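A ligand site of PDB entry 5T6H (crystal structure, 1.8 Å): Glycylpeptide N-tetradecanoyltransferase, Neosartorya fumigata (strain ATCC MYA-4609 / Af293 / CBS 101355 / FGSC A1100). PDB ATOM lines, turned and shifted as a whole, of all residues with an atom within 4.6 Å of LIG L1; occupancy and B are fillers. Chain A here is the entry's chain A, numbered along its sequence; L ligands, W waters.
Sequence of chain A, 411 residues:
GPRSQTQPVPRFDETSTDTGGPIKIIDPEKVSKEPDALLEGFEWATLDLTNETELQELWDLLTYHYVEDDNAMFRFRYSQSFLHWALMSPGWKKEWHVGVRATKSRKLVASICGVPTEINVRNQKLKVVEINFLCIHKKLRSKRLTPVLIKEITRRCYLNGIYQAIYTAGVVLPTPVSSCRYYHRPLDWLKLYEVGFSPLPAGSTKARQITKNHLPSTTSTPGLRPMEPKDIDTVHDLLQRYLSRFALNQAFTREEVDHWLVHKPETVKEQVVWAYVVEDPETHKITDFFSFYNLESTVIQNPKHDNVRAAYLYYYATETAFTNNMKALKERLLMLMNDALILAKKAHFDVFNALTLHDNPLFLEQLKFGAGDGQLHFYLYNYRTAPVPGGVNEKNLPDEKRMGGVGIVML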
ATOM      1  N   TYR A  66       8.325  -6.811 -21.920  1.00  0.00           N
ATOM      2  CA  TYR A  66       7.272  -6.853 -20.925  1.00  0.00           C
ATOM      3  C   TYR A  66       7.797  -6.529 -19.525  1.00  0.00           C
ATOM      4  O   TYR A  66       8.934  -6.005 -19.375  1.00  0.00           O
ATOM      5  CB  TYR A  66       6.488  -8.195 -21.015  1.00  0.00           C
ATOM      6  CG  TYR A  66       5.062  -8.110 -20.485  1.00  0.00           C
ATOM      7  CD1 TYR A  66       4.232  -7.075 -20.872  1.00  0.00           C
ATOM      8  CD2 TYR A  66       4.566  -9.054 -19.569  1.00  0.00           C
ATOM      9  CE1 TYR A  66       2.925  -6.986 -20.372  1.00  0.00           C
ATOM     10  CE2 TYR A  66       3.300  -8.958 -19.064  1.00  0.00           C
ATOM     11  CZ  TYR A  66       2.478  -7.921 -19.457  1.00  0.00           C
ATOM     12  OH  TYR A  66       1.181  -7.839 -18.965  1.00  0.00           O
ATOM     13  N   VAL A  67       7.020  -6.805 -18.519  1.00  0.00           N
ATOM     14  CA  VAL A  67       7.272  -6.330 -17.125  1.00  0.00           C
ATOM     15  C   VAL A  67       8.618  -6.792 -16.579  1.00  0.00           C
ATOM     16  O   VAL A  67       8.898  -7.978 -16.543  1.00  0.00           O
ATOM     17  CB  VAL A  67       6.170  -6.870 -16.208  1.00  0.00           C
ATOM     18  CG1 VAL A  67       6.422  -6.474 -14.780  1.00  0.00           C
ATOM     19  CG2 VAL A  67       4.803  -6.424 -16.687  1.00  0.00           C
ATOM     20  N   GLU A  68       9.415  -5.831 -16.087  1.00  0.00           N
ATOM     21  CA  GLU A  68      10.672  -6.107 -15.346  1.00  0.00           C
ATOM     22  C   GLU A  68      10.584  -5.627 -13.901  1.00  0.00           C
ATOM     23  O   GLU A  68       9.743  -4.759 -13.562  1.00  0.00           O
ATOM     24  CB  GLU A  68      11.872  -5.390 -16.013  1.00  0.00           C
ATOM     25  CG  GLU A  68      12.116  -5.776 -17.437  1.00  0.00           C
ATOM     26  CD  GLU A  68      13.231  -4.972 -18.096  1.00  0.00           C
ATOM     27  OE1 GLU A  68      13.897  -4.155 -17.393  1.00  0.00           O
ATOM     28  OE2 GLU A  68      13.428  -5.125 -19.317  1.00  0.00           O
ATOM     29  N   ASP A  69      11.403  -6.198 -13.021  1.00  0.00           N
ATOM     30  CA  ASP A  69      11.463  -5.693 -11.628  1.00  0.00           C
ATOM     31  C   ASP A  69      12.211  -4.359 -11.638  1.00  0.00           C
ATOM     32  O   ASP A  69      12.871  -3.994 -12.624  1.00  0.00           O
ATOM     33  CB  ASP A  69      12.243  -6.664 -10.739  1.00  0.00           C
ATOM     34  CG  ASP A  69      13.685  -6.754 -11.116  1.00  0.00           C
ATOM     35  OD1 ASP A  69      14.008  -7.004 -12.314  1.00  0.00           O
ATOM     36  OD2 ASP A  69      14.560  -6.511 -10.238  1.00  0.00           O
ATOM     37  N   PHE A  74      15.110  -9.189 -13.655  1.00  0.00           N
ATOM     38  CA  PHE A  74      14.200 -10.209 -14.150  1.00  0.00           C
ATOM     39  C   PHE A  74      13.145  -9.608 -15.071  1.00  0.00           C
ATOM     40  O   PHE A  74      12.727  -8.488 -14.874  1.00  0.00           O
ATOM     41  CB  PHE A  74      13.462 -10.908 -12.993  1.00  0.00           C
ATOM     42  CG  PHE A  74      14.377 -11.386 -11.917  1.00  0.00           C
ATOM     43  CD1 PHE A  74      15.170 -12.504 -12.116  1.00  0.00           C
ATOM     44  CD2 PHE A  74      14.425 -10.715 -10.709  1.00  0.00           C
ATOM     45  CE1 PHE A  74      16.066 -12.943 -11.099  1.00  0.00           C
ATOM     46  CE2 PHE A  74      15.290 -11.139  -9.692  1.00  0.00           C
ATOM     47  CZ  PHE A  74      16.110 -12.240  -9.899  1.00  0.00           C
ATOM     48  N   ARG A  75      12.677 -10.418 -16.019  1.00  0.00           N
ATOM     49  CA  ARG A  75      11.559  -9.969 -16.898  1.00  0.00           C
ATOM     50  C   ARG A  75      10.611 -11.152 -17.053  1.00  0.00           C
ATOM     51  O   ARG A  75      11.063 -12.254 -17.366  1.00  0.00           O
ATOM     52  CB  ARG A  75      12.061  -9.513 -18.239  1.00  0.00           C
ATOM     53  CG  ARG A  75      11.016  -8.826 -19.113  1.00  0.00           C
ATOM     54  CD  ARG A  75      11.516  -8.412 -20.505  1.00  0.00           C
ATOM     55  NE  ARG A  75      12.713  -7.640 -20.414  1.00  0.00           N
ATOM     56  CZ  ARG A  75      13.909  -8.017 -20.854  1.00  0.00           C
ATOM     57  NH1 ARG A  75      14.051  -9.128 -21.573  1.00  0.00           N
ATOM     58  NH2 ARG A  75      14.929  -7.222 -20.661  1.00  0.00           N
ATOM     59  N   PHE A  76       9.312 -10.919 -16.871  1.00  0.00           N
ATOM     60  CA  PHE A  76       8.347 -12.019 -17.098  1.00  0.00           C
ATOM     61  C   PHE A  76       8.564 -12.615 -18.473  1.00  0.00           C
ATOM     62  O   PHE A  76       8.838 -11.910 -19.468  1.00  0.00           O
ATOM     63  CB  PHE A  76       6.905 -11.571 -16.932  1.00  0.00           C
ATOM     64  CG  PHE A  76       6.490 -11.372 -15.485  1.00  0.00           C
ATOM     65  CD1 PHE A  76       6.923 -12.263 -14.509  1.00  0.00           C
ATOM     66  CD2 PHE A  76       5.739 -10.270 -15.103  1.00  0.00           C
ATOM     67  CE1 PHE A  76       6.571 -12.082 -13.190  1.00  0.00           C
ATOM     68  CE2 PHE A  76       5.377 -10.085 -13.762  1.00  0.00           C
ATOM     69  CZ  PHE A  76       5.816 -11.002 -12.805  1.00  0.00           C
ATOM     70  N   ASN A 132      -5.022  -7.284 -20.251  1.00  0.00           N
ATOM     71  CA  ASN A 132      -3.714  -7.787 -19.907  1.00  0.00           C
ATOM     72  C   ASN A 132      -2.778  -7.570 -21.118  1.00  0.00           C
ATOM     73  O   ASN A 132      -3.227  -7.296 -22.229  1.00  0.00           O
ATOM     74  CB  ASN A 132      -3.828  -9.266 -19.538  1.00  0.00           C
ATOM     75  CG  ASN A 132      -2.794  -9.740 -18.542  1.00  0.00           C
ATOM     76  OD1 ASN A 132      -1.803  -9.080 -18.257  1.00  0.00           O
ATOM     77  ND2 ASN A 132      -3.036 -10.929 -18.019  1.00  0.00           N
ATOM     78  N   THR A 168      -5.366  -5.840 -13.493  1.00  0.00           N
ATOM     79  CA  THR A 168      -4.385  -5.578 -12.456  1.00  0.00           C
ATOM     80  C   THR A 168      -3.182  -4.866 -13.036  1.00  0.00           C
ATOM     81  O   THR A 168      -2.905  -4.963 -14.267  1.00  0.00           O
ATOM     82  CB  THR A 168      -3.902  -6.863 -11.757  1.00  0.00           C
ATOM     83  OG1 THR A 168      -3.419  -7.786 -12.734  1.00  0.00           O
ATOM     84  CG2 THR A 168      -5.053  -7.532 -11.024  1.00  0.00           C
ATOM     85  N   ALA A 169      -2.438  -4.177 -12.184  1.00  0.00           N
ATOM     86  CA  ALA A 169      -1.163  -3.538 -12.583  1.00  0.00           C
ATOM     87  C   ALA A 169      -0.300  -3.330 -11.366  1.00  0.00           C
ATOM     88  O   ALA A 169      -0.795  -3.270 -10.246  1.00  0.00           O
ATOM     89  CB  ALA A 169      -1.423  -2.181 -13.250  1.00  0.00           C
ATOM     90  N   GLY A 170       1.018  -3.237 -11.559  1.00  0.00           N
ATOM     91  CA  GLY A 170       1.888  -2.936 -10.446  1.00  0.00           C
ATOM     92  C   GLY A 170       1.950  -1.459 -10.124  1.00  0.00           C
ATOM     93  O   GLY A 170       2.428  -1.067  -9.078  1.00  0.00           O
ATOM     94  N   TYR A 182       2.687  -9.574  -2.870  1.00  0.00           N
ATOM     95  CA  TYR A 182       3.312 -10.800  -3.363  1.00  0.00           C
ATOM     96  C   TYR A 182       4.130 -11.523  -2.275  1.00  0.00           C
ATOM     97  O   TYR A 182       4.810 -10.871  -1.503  1.00  0.00           O
ATOM     98  CB  TYR A 182       4.218 -10.513  -4.535  1.00  0.00           C
ATOM     99  CG  TYR A 182       3.531 -10.397  -5.899  1.00  0.00           C
ATOM    100  CD1 TYR A 182       3.089 -11.529  -6.591  1.00  0.00           C
ATOM    101  CD2 TYR A 182       3.337  -9.164  -6.497  1.00  0.00           C
ATOM    102  CE1 TYR A 182       2.486 -11.411  -7.830  1.00  0.00           C
ATOM    103  CE2 TYR A 182       2.746  -9.048  -7.720  1.00  0.00           C
ATOM    104  CZ  TYR A 182       2.296 -10.156  -8.379  1.00  0.00           C
ATOM    105  OH  TYR A 182       1.716 -10.006  -9.609  1.00  0.00           O
ATOM    106  N   HIS A 184       6.702 -15.223  -1.667  1.00  0.00           N
ATOM    107  CA  HIS A 184       7.550 -16.097  -2.470  1.00  0.00           C
ATOM    108  C   HIS A 184       8.131 -17.223  -1.649  1.00  0.00           C
ATOM    109  O   HIS A 184       8.861 -16.959  -0.682  1.00  0.00           O
ATOM    110  CB  HIS A 184       8.673 -15.315  -3.111  1.00  0.00           C
ATOM    111  CG  HIS A 184       8.239 -14.086  -3.852  1.00  0.00           C
ATOM    112  ND1 HIS A 184       7.796 -14.127  -5.149  1.00  0.00           N
ATOM    113  CD2 HIS A 184       8.181 -12.785  -3.470  1.00  0.00           C
ATOM    114  CE1 HIS A 184       7.495 -12.897  -5.549  1.00  0.00           C
ATOM    115  NE2 HIS A 184       7.715 -12.064  -4.557  1.00  0.00           N
ATOM    116  N   PHE A 197      17.891 -13.315  -6.427  1.00  0.00           N
ATOM    117  CA  PHE A 197      16.573 -13.128  -5.850  1.00  0.00           C
ATOM    118  C   PHE A 197      16.506 -13.318  -4.328  1.00  0.00           C
ATOM    119  O   PHE A 197      15.853 -12.534  -3.645  1.00  0.00           O
ATOM    120  CB  PHE A 197      15.569 -14.054  -6.496  1.00  0.00           C
ATOM    121  CG  PHE A 197      14.156 -13.866  -5.958  1.00  0.00           C
ATOM    122  CD1 PHE A 197      13.397 -12.767  -6.347  1.00  0.00           C
ATOM    123  CD2 PHE A 197      13.656 -14.725  -4.997  1.00  0.00           C
ATOM    124  CE1 PHE A 197      12.121 -12.562  -5.827  1.00  0.00           C
ATOM    125  CE2 PHE A 197      12.382 -14.543  -4.467  1.00  0.00           C
ATOM    126  CZ  PHE A 197      11.608 -13.462  -4.883  1.00  0.00           C
ATOM    127  N   SER A 297      10.485 -16.394 -15.520  1.00  0.00           N
ATOM    128  CA  SER A 297      11.082 -15.081 -15.668  1.00  0.00           C
ATOM    129  C   SER A 297      12.449 -15.219 -16.295  1.00  0.00           C
ATOM    130  O   SER A 297      13.234 -16.072 -15.875  1.00  0.00           O
ATOM    131  CB  SER A 297      11.203 -14.326 -14.347  1.00  0.00           C
ATOM    132  OG  SER A 297       9.945 -13.788 -13.939  1.00  0.00           O
ATOM    133  N   TYR A 312       2.878 -20.225  -9.811  1.00  0.00           N
ATOM    134  CA  TYR A 312       2.031 -19.261  -9.105  1.00  0.00           C
ATOM    135  C   TYR A 312       0.788 -19.987  -8.597  1.00  0.00           C
ATOM    136  O   TYR A 312       0.094 -20.641  -9.371  1.00  0.00           O
ATOM    137  CB  TYR A 312       1.605 -18.109 -10.035  1.00  0.00           C
ATOM    138  CG  TYR A 312       2.715 -17.114 -10.336  1.00  0.00           C
ATOM    139  CD1 TYR A 312       3.779 -17.452 -11.167  1.00  0.00           C
ATOM    140  CD2 TYR A 312       2.679 -15.845  -9.820  1.00  0.00           C
ATOM    141  CE1 TYR A 312       4.784 -16.551 -11.441  1.00  0.00           C
ATOM    142  CE2 TYR A 312       3.724 -14.929 -10.087  1.00  0.00           C
ATOM    143  CZ  TYR A 312       4.759 -15.298 -10.884  1.00  0.00           C
ATOM    144  OH  TYR A 312       5.784 -14.370 -11.121  1.00  0.00           O
ATOM    145  N   ASP A 373       8.698  -7.649  -2.348  1.00  0.00           N
ATOM    146  CA  ASP A 373       8.654  -6.213  -2.518  1.00  0.00           C
ATOM    147  C   ASP A 373       7.438  -5.763  -3.321  1.00  0.00           C
ATOM    148  O   ASP A 373       7.043  -4.613  -3.268  1.00  0.00           O
ATOM    149  CB  ASP A 373       9.925  -5.756  -3.216  1.00  0.00           C
ATOM    150  CG  ASP A 373      11.173  -6.100  -2.396  1.00  0.00           C
ATOM    151  OD1 ASP A 373      11.084  -5.987  -1.134  1.00  0.00           O
ATOM    152  OD2 ASP A 373      12.212  -6.419  -3.015  1.00  0.00           O
ATOM    153  N   GLY A 374       6.858  -6.693  -4.059  1.00  0.00           N
ATOM    154  CA  GLY A 374       5.814  -6.383  -5.016  1.00  0.00           C
ATOM    155  C   GLY A 374       4.420  -6.245  -4.407  1.00  0.00           C
ATOM    156  O   GLY A 374       4.035  -7.018  -3.532  1.00  0.00           O
ATOM    157  N   GLN A 375       3.680  -5.265  -4.919  1.00  0.00           N
ATOM    158  CA  GLN A 375       2.255  -5.144  -4.694  1.00  0.00           C
ATOM    159  C   GLN A 375       1.518  -5.233  -6.055  1.00  0.00           C
ATOM    160  O   GLN A 375       1.988  -4.692  -7.048  1.00  0.00           O
ATOM    161  CB  GLN A 375       1.950  -3.817  -4.066  1.00  0.00           C
ATOM    162  CG  GLN A 375       0.729  -3.770  -3.202  1.00  0.00           C
ATOM    163  CD  GLN A 375       0.945  -4.391  -1.824  1.00  0.00           C
ATOM    164  OE1 GLN A 375       2.026  -4.910  -1.544  1.00  0.00           O
ATOM    165  NE2 GLN A 375      -0.096  -4.332  -0.975  1.00  0.00           N
ATOM    166  N   LEU A 376       0.370  -5.881  -6.050  1.00  0.00           N
ATOM    167  CA  LEU A 376      -0.485  -5.905  -7.251  1.00  0.00           C
ATOM    168  C   LEU A 376      -1.783  -5.179  -6.954  1.00  0.00           C
ATOM    169  O   LEU A 376      -2.497  -5.537  -6.001  1.00  0.00           O
ATOM    170  CB  LEU A 376      -0.775  -7.310  -7.669  1.00  0.00           C
ATOM    171  CG  LEU A 376      -1.400  -7.472  -9.033  1.00  0.00           C
ATOM    172  CD1 LEU A 376      -0.479  -6.960 -10.128  1.00  0.00           C
ATOM    173  CD2 LEU A 376      -1.794  -8.928  -9.321  1.00  0.00           C
ATOM    174  N   MET A 410      -5.625 -12.910 -11.505  1.00  0.00           N
ATOM    175  CA  MET A 410      -5.404 -12.605 -12.899  1.00  0.00           C
ATOM    176  C   MET A 410      -3.942 -12.950 -13.268  1.00  0.00           C
ATOM    177  O   MET A 410      -3.064 -12.962 -12.405  1.00  0.00           O
ATOM    178  CB  MET A 410      -5.701 -11.145 -13.201  1.00  0.00           C
ATOM    179  CG  MET A 410      -7.115 -10.727 -12.790  1.00  0.00           C
ATOM    180  SD  MET A 410      -7.600  -9.134 -13.484  1.00  0.00           S
ATOM    181  CE  MET A 410      -7.555  -9.511 -15.196  1.00  0.00           C
ATOM    182  N   LEU A 411      -3.721 -13.278 -14.529  1.00  0.00           N
ATOM    183  CA  LEU A 411      -2.469 -13.879 -14.987  1.00  0.00           C
ATOM    184  C   LEU A 411      -1.339 -12.896 -15.318  1.00  0.00           C
ATOM    185  O   LEU A 411      -1.574 -11.742 -15.696  1.00  0.00           O
ATOM    186  CB  LEU A 411      -2.737 -14.772 -16.199  1.00  0.00           C
ATOM    187  CG  LEU A 411      -3.751 -15.871 -15.916  1.00  0.00           C
ATOM    188  CD1 LEU A 411      -4.079 -16.639 -17.189  1.00  0.00           C
ATOM    189  CD2 LEU A 411      -3.281 -16.815 -14.845  1.00  0.00           C
ATOM    190  OXT LEU A 411      -0.171 -13.310 -15.304  1.00  0.00           O
HETATM  191  C1  LIG L   1       0.936  -9.176 -13.131  1.00  0.00           C
HETATM  192  C2  LIG L   1      -0.546  -9.343 -13.297  1.00  0.00           C
HETATM  193  N1  LIG L   1      -1.066  -9.021 -14.616  1.00  0.00           N
HETATM  194  C3  LIG L   1      -0.711  -7.613 -14.886  1.00  0.00           C
HETATM  195  C4  LIG L   1       0.771  -7.316 -14.752  1.00  0.00           C
HETATM  196  N2  LIG L   1       1.288  -7.787 -13.464  1.00  0.00           N
HETATM  197  C5  LIG L   1       2.297  -7.059 -12.858  1.00  0.00           C
HETATM  198  C6  LIG L   1       3.081  -7.581 -11.834  1.00  0.00           C
HETATM  199  N3  LIG L   1       2.563  -5.873 -13.400  1.00  0.00           N
HETATM  200  C7  LIG L   1       3.496  -5.118 -12.899  1.00  0.00           C
HETATM  201  C8  LIG L   1       4.280  -5.538 -11.869  1.00  0.00           C
HETATM  202  C9  LIG L   1       4.025  -6.779 -11.300  1.00  0.00           C
HETATM  203  C10 LIG L   1       4.878  -7.202 -10.299  1.00  0.00           C
HETATM  204  C11 LIG L   1       5.119  -8.565 -10.064  1.00  0.00           C
HETATM  205  C12 LIG L   1       6.049  -8.964  -9.122  1.00  0.00           C
HETATM  206 CL1  LIG L   1       6.235 -10.647  -8.885  1.00  0.00          CL
HETATM  207  C13 LIG L   1       5.578  -6.238  -9.577  1.00  0.00           C
HETATM  208  C14 LIG L   1       6.478  -6.618  -8.599  1.00  0.00           C
HETATM  209 CL2  LIG L   1       7.283  -5.312  -7.738  1.00  0.00          CL
HETATM  210  C15 LIG L   1       6.699  -7.970  -8.334  1.00  0.00           C
HETATM  211  O1  LIG L   1       7.659  -8.360  -7.416  1.00  0.00           O
HETATM  212  C16 LIG L   1       8.954  -8.077  -8.104  1.00  0.00           C
HETATM  213  C17 LIG L   1       9.168  -8.547  -9.431  1.00  0.00           C
HETATM  214  C18 LIG L   1       8.801  -7.747 -10.528  1.00  0.00           C
HETATM  215  C19 LIG L   1       8.965  -8.212 -11.816  1.00  0.00           C
HETATM  216  C20 LIG L   1       9.580  -9.455 -12.009  1.00  0.00           C
HETATM  217  C21 LIG L   1       9.789  -9.949 -13.437  1.00  0.00           C
HETATM  218  N4  LIG L   1       9.953 -10.193 -10.965  1.00  0.00           N
HETATM  219  C22 LIG L   1       9.754  -9.782  -9.691  1.00  0.00           C
HETATM  220  C23 LIG L   1      10.210 -10.662  -8.529  1.00  0.00           C
HETATM  221  S1  LG2 L   2      -0.416  -4.170 -16.622  1.00  0.00           S
HETATM  222  C1  LG2 L   2       1.110  -4.565 -17.501  1.00  0.00           C
HETATM  223  C2  LG2 L   2       1.654  -3.287 -18.067  1.00  0.00           C
HETATM  224  N1  LG2 L   2       2.820  -3.613 -18.863  1.00  0.00           N
HETATM  225  C3  LG2 L   2       4.111  -3.490 -18.524  1.00  0.00           C
HETATM  226  O1  LG2 L   2       4.458  -3.072 -17.400  1.00  0.00           O
HETATM  227  C4  LG2 L   2       5.129  -3.842 -19.537  1.00  0.00           C
HETATM  228  C5  LG2 L   2       6.382  -2.945 -19.458  1.00  0.00           C
HETATM  229  N2  LG2 L   2       6.014  -1.576 -19.670  1.00  0.00           N
HETATM  230  C6  LG2 L   2       5.524  -1.048 -20.798  1.00  0.00           C
HETATM  231  O2  LG2 L   2       5.339  -1.732 -21.836  1.00  0.00           O
HETATM  232  C7  LG2 L   2       5.188   0.414 -20.813  1.00  0.00           C
HETATM  233  O3  LG2 L   2       5.934   1.137 -19.809  1.00  0.00           O
HETATM  234  C8  LG2 L   2       3.678   0.662 -20.630  1.00  0.00           C
HETATM  235  C9  LG2 L   2       3.460   2.182 -20.467  1.00  0.00           C
HETATM  236  C10 LG2 L   2       3.089  -0.036 -19.399  1.00  0.00           C
HETATM  237  C11 LG2 L   2       2.979   0.197 -21.874  1.00  0.00           C
HETATM  238  N3  LG2 L   2      -1.711   0.426 -16.902  1.00  0.00           N
HETATM  239  O4  LG2 L   2       2.551   5.534 -23.361  1.00  0.00           O
HETATM  240  P1  LG2 L   2       3.013   6.299 -22.117  1.00  0.00           P
HETATM  241  C12 LG2 L   2      -0.193   5.284 -17.934  1.00  0.00           C
HETATM  242  C13 LG2 L   2      -2.467   1.480 -17.270  1.00  0.00           C
HETATM  243  O5  LG2 L   2       3.906   7.505 -22.312  1.00  0.00           O
HETATM  244  P2  LG2 L   2       4.870   4.197 -21.436  1.00  0.00           P
HETATM  245  C14 LG2 L   2      -1.610  -4.488 -17.774  1.00  0.00           C
HETATM  246  O6  LG2 L   2      -1.356  -5.107 -18.823  1.00  0.00           O
HETATM  247  C15 LG2 L   2       0.560   6.355 -17.133  1.00  0.00           C
HETATM  248  O7  LG2 L   2       0.084   6.469 -15.783  1.00  0.00           O
HETATM  249  N4  LG2 L   2      -1.911   2.710 -17.504  1.00  0.00           N
HETATM  250  O8  LG2 L   2       3.745   5.309 -21.063  1.00  0.00           O
HETATM  251  C16 LG2 L   2      -2.999  -3.983 -17.532  1.00  0.00           C
HETATM  252  C17 LG2 L   2       0.376   7.605 -17.929  1.00  0.00           C
HETATM  253  O9  LG2 L   2      -0.934   8.075 -17.701  1.00  0.00           O
HETATM  254  P3  LG2 L   2      -1.368   9.615 -17.507  1.00  0.00           P
HETATM  255  C18 LG2 L   2      -0.573   2.860 -17.379  1.00  0.00           C
HETATM  256  O10 LG2 L   2       5.486   4.494 -22.760  1.00  0.00           O
HETATM  257  C19 LG2 L   2      -3.243  -2.763 -18.384  1.00  0.00           C
HETATM  258  C20 LG2 L   2       0.405   7.060 -19.358  1.00  0.00           C
HETATM  259  O11 LG2 L   2       0.138   5.619 -19.274  1.00  0.00           O
HETATM  260  C21 LG2 L   2       0.208   1.778 -17.006  1.00  0.00           C
HETATM  261  O12 LG2 L   2       5.723   3.983 -20.233  1.00  0.00           O
HETATM  262  C22 LG2 L   2      -4.611  -2.126 -18.113  1.00  0.00           C
HETATM  263  C23 LG2 L   2       1.706   7.305 -20.052  1.00  0.00           C
HETATM  264  O13 LG2 L   2       1.687   6.639 -21.321  1.00  0.00           O
HETATM  265  C24 LG2 L   2      -0.397   0.553 -16.784  1.00  0.00           C
HETATM  266  N5  LG2 L   2       0.351  -0.516 -16.398  1.00  0.00           N
HETATM  267  O14 LG2 L   2       3.955   2.836 -21.601  1.00  0.00           O
HETATM  268  C25 LG2 L   2      -4.855  -0.882 -18.990  1.00  0.00           C
HETATM  269  N6  LG2 L   2       1.507   2.197 -16.976  1.00  0.00           N
HETATM  270  O15 LG2 L   2      -2.058  10.062 -18.877  1.00  0.00           O
HETATM  271  C26 LG2 L   2      -6.181  -0.147 -18.709  1.00  0.00           C
HETATM  272  C27 LG2 L   2       1.531   3.536 -17.282  1.00  0.00           C
HETATM  273  O16 LG2 L   2      -0.008  10.383 -17.189  1.00  0.00           O
HETATM  274  C28 LG2 L   2      -7.429  -0.923 -19.104  1.00  0.00           C
HETATM  275  N7  LG2 L   2       0.241   3.909 -17.571  1.00  0.00           N
HETATM  276  O17 LG2 L   2      -2.473   9.641 -16.367  1.00  0.00           O
HETATM  277  C29 LG2 L   2      -8.669  -0.031 -19.035  1.00  0.00           C
HETATM  278  C30 LG2 L   2      -9.929  -0.768 -19.482  1.00  0.00           C
HETATM  279  C31 LG2 L   2      -9.870  -0.943 -20.991  1.00  0.00           C
HETATM  280  C32 LG2 L   2     -11.037  -1.753 -21.515  1.00  0.00           C
HETATM  281  C33 LG2 L   2     -12.415  -1.096 -21.197  1.00  0.00           C
HETATM  282  C34 LG2 L   2     -13.504  -1.972 -21.798  1.00  0.00           C
HETATM  283  C35 LG2 L   2     -14.909  -1.549 -21.408  1.00  0.00           C
HETATM  284  O   HOH W   1      -3.507  -9.603 -15.029  1.00  0.00           O
HETATM  285  O   HOH W   2       8.132  -3.169  -9.582  1.00  0.00           O
HETATM  286  O   HOH W   3      11.820  -9.001  -6.130  1.00  0.00           O
HETATM  287  O   HOH W   4       1.664  -3.290 -14.417  1.00  0.00           O
HETATM  288  O   HOH W   5       7.772  -9.356  -5.161  1.00  0.00           O
HETATM  289  O   HOH W   6       7.790  -2.800  -5.648  1.00  0.00           O
HETATM  290  O   HOH W   7      10.250  -4.316  -8.751  1.00  0.00           O
HETATM  291  O   HOH W   8       0.568  -9.702 -17.139  1.00  0.00           O
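Water W5 lies within hydrogen-bond range of an oxygen (O1) of LIG L1, a ring nitrogen (NE2) of His 184, the backbone NH (N) of Gly 374 and the backbone NH (N) of Asp 373.
Water W1 lies within hydrogen-bond range of a nitrogen (N1) of LIG L1 (2.5 Å), the side-chain hydroxyl of Thr 168 (2.9 Å), the chain-end carboxylate of Leu 411 (3.0 Å) and the side-chain amide nitrogen of Asn 132 (3.3 Å).
Water W4 lies within hydrogen-bond range of N3 of LIG L1 (2.9 Å), N of Gly 170 (2.9 Å) and S1 of LG2 L2 (3.2 Å).
Water W8 lies within hydrogen-bond range of OH of Tyr 66, OD1 of Asn 132, N1 of LIG L1 and O of Leu 411.
Val 67 touches LIG L1 (CG1 to C8, 3.7 Å).
Glu 68 touches LIG L1.
Asp 69 touches LIG L1 (N to C19, 3.4 Å).
Phe 74 touches LIG L1 (O to C21, 3.6 Å).
Arg 75 touches LIG L1.
N of Phe 76 touches C21 of LIG L1, 3.6 Å away.
Asn 132 touches LIG L1 (OD1 to N1, 3.7 Å).
Gly 170 touches LIG L1 (N to C7, 3.4 Å).
Tyr 182 touches LIG L1.
Phe 197 touches LIG L1 (CE1 to C23, 3.8 Å).
OG of Ser 297 touches C21 of LIG L1, at 3.9 Å.
Gly 374 touches LIG L1 (CA to CL2, 3.3 Å).
CD1 of Leu 376 touches N2 of LIG L1 (3.9 Å).
Hydrophobic or aromatic side chains within 4 Å of LIG L1: Val 67, Phe 74, Phe 76, Tyr 182, Phe 197 and Leu 376.
15 residues have an atom within 4 Å of LIG L1: Val 67, Glu 68, Asp 69, Phe 74, Arg 75, Phe 76, Asn 132, Thr 168, Gly 170, Tyr 182, Phe 197, Ser 297, Gly 374, Leu 376 and Leu 411.
The nearest printed residue that does not touch LIG L1 is His 184 (4.2 Å).
N1 of LIG L1 is in salt-bridge range of O of Leu 411.
N1 of LIG L1 sits at hydrogen-bond distance from OG1 of Thr 168.
The chain-end carboxylate of Leu 411 lies within hydrogen-bond range of the side-chain amide nitrogen of Asn 132 (2.9 Å).
The backbone carbonyl oxygen (O) of Gly 374 lies within hydrogen-bond range of the backbone NH (N) of Tyr 182 (3.0 Å).
The side-chain carboxylate (OD1) of Asp 69 sits at hydrogen-bond distance from the backbone NH (N) of Phe 74 (2.8 Å).
N of Phe 76 lies within hydrogen-bond range of O of Val 67.
The side-chain carboxylate of Glu 68 lies within salt-bridge range of the guanidinium group of Arg 75.
OD1 of Asn 132 is in hydrogen-bond range of OH of Tyr 66 (3.3 Å).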
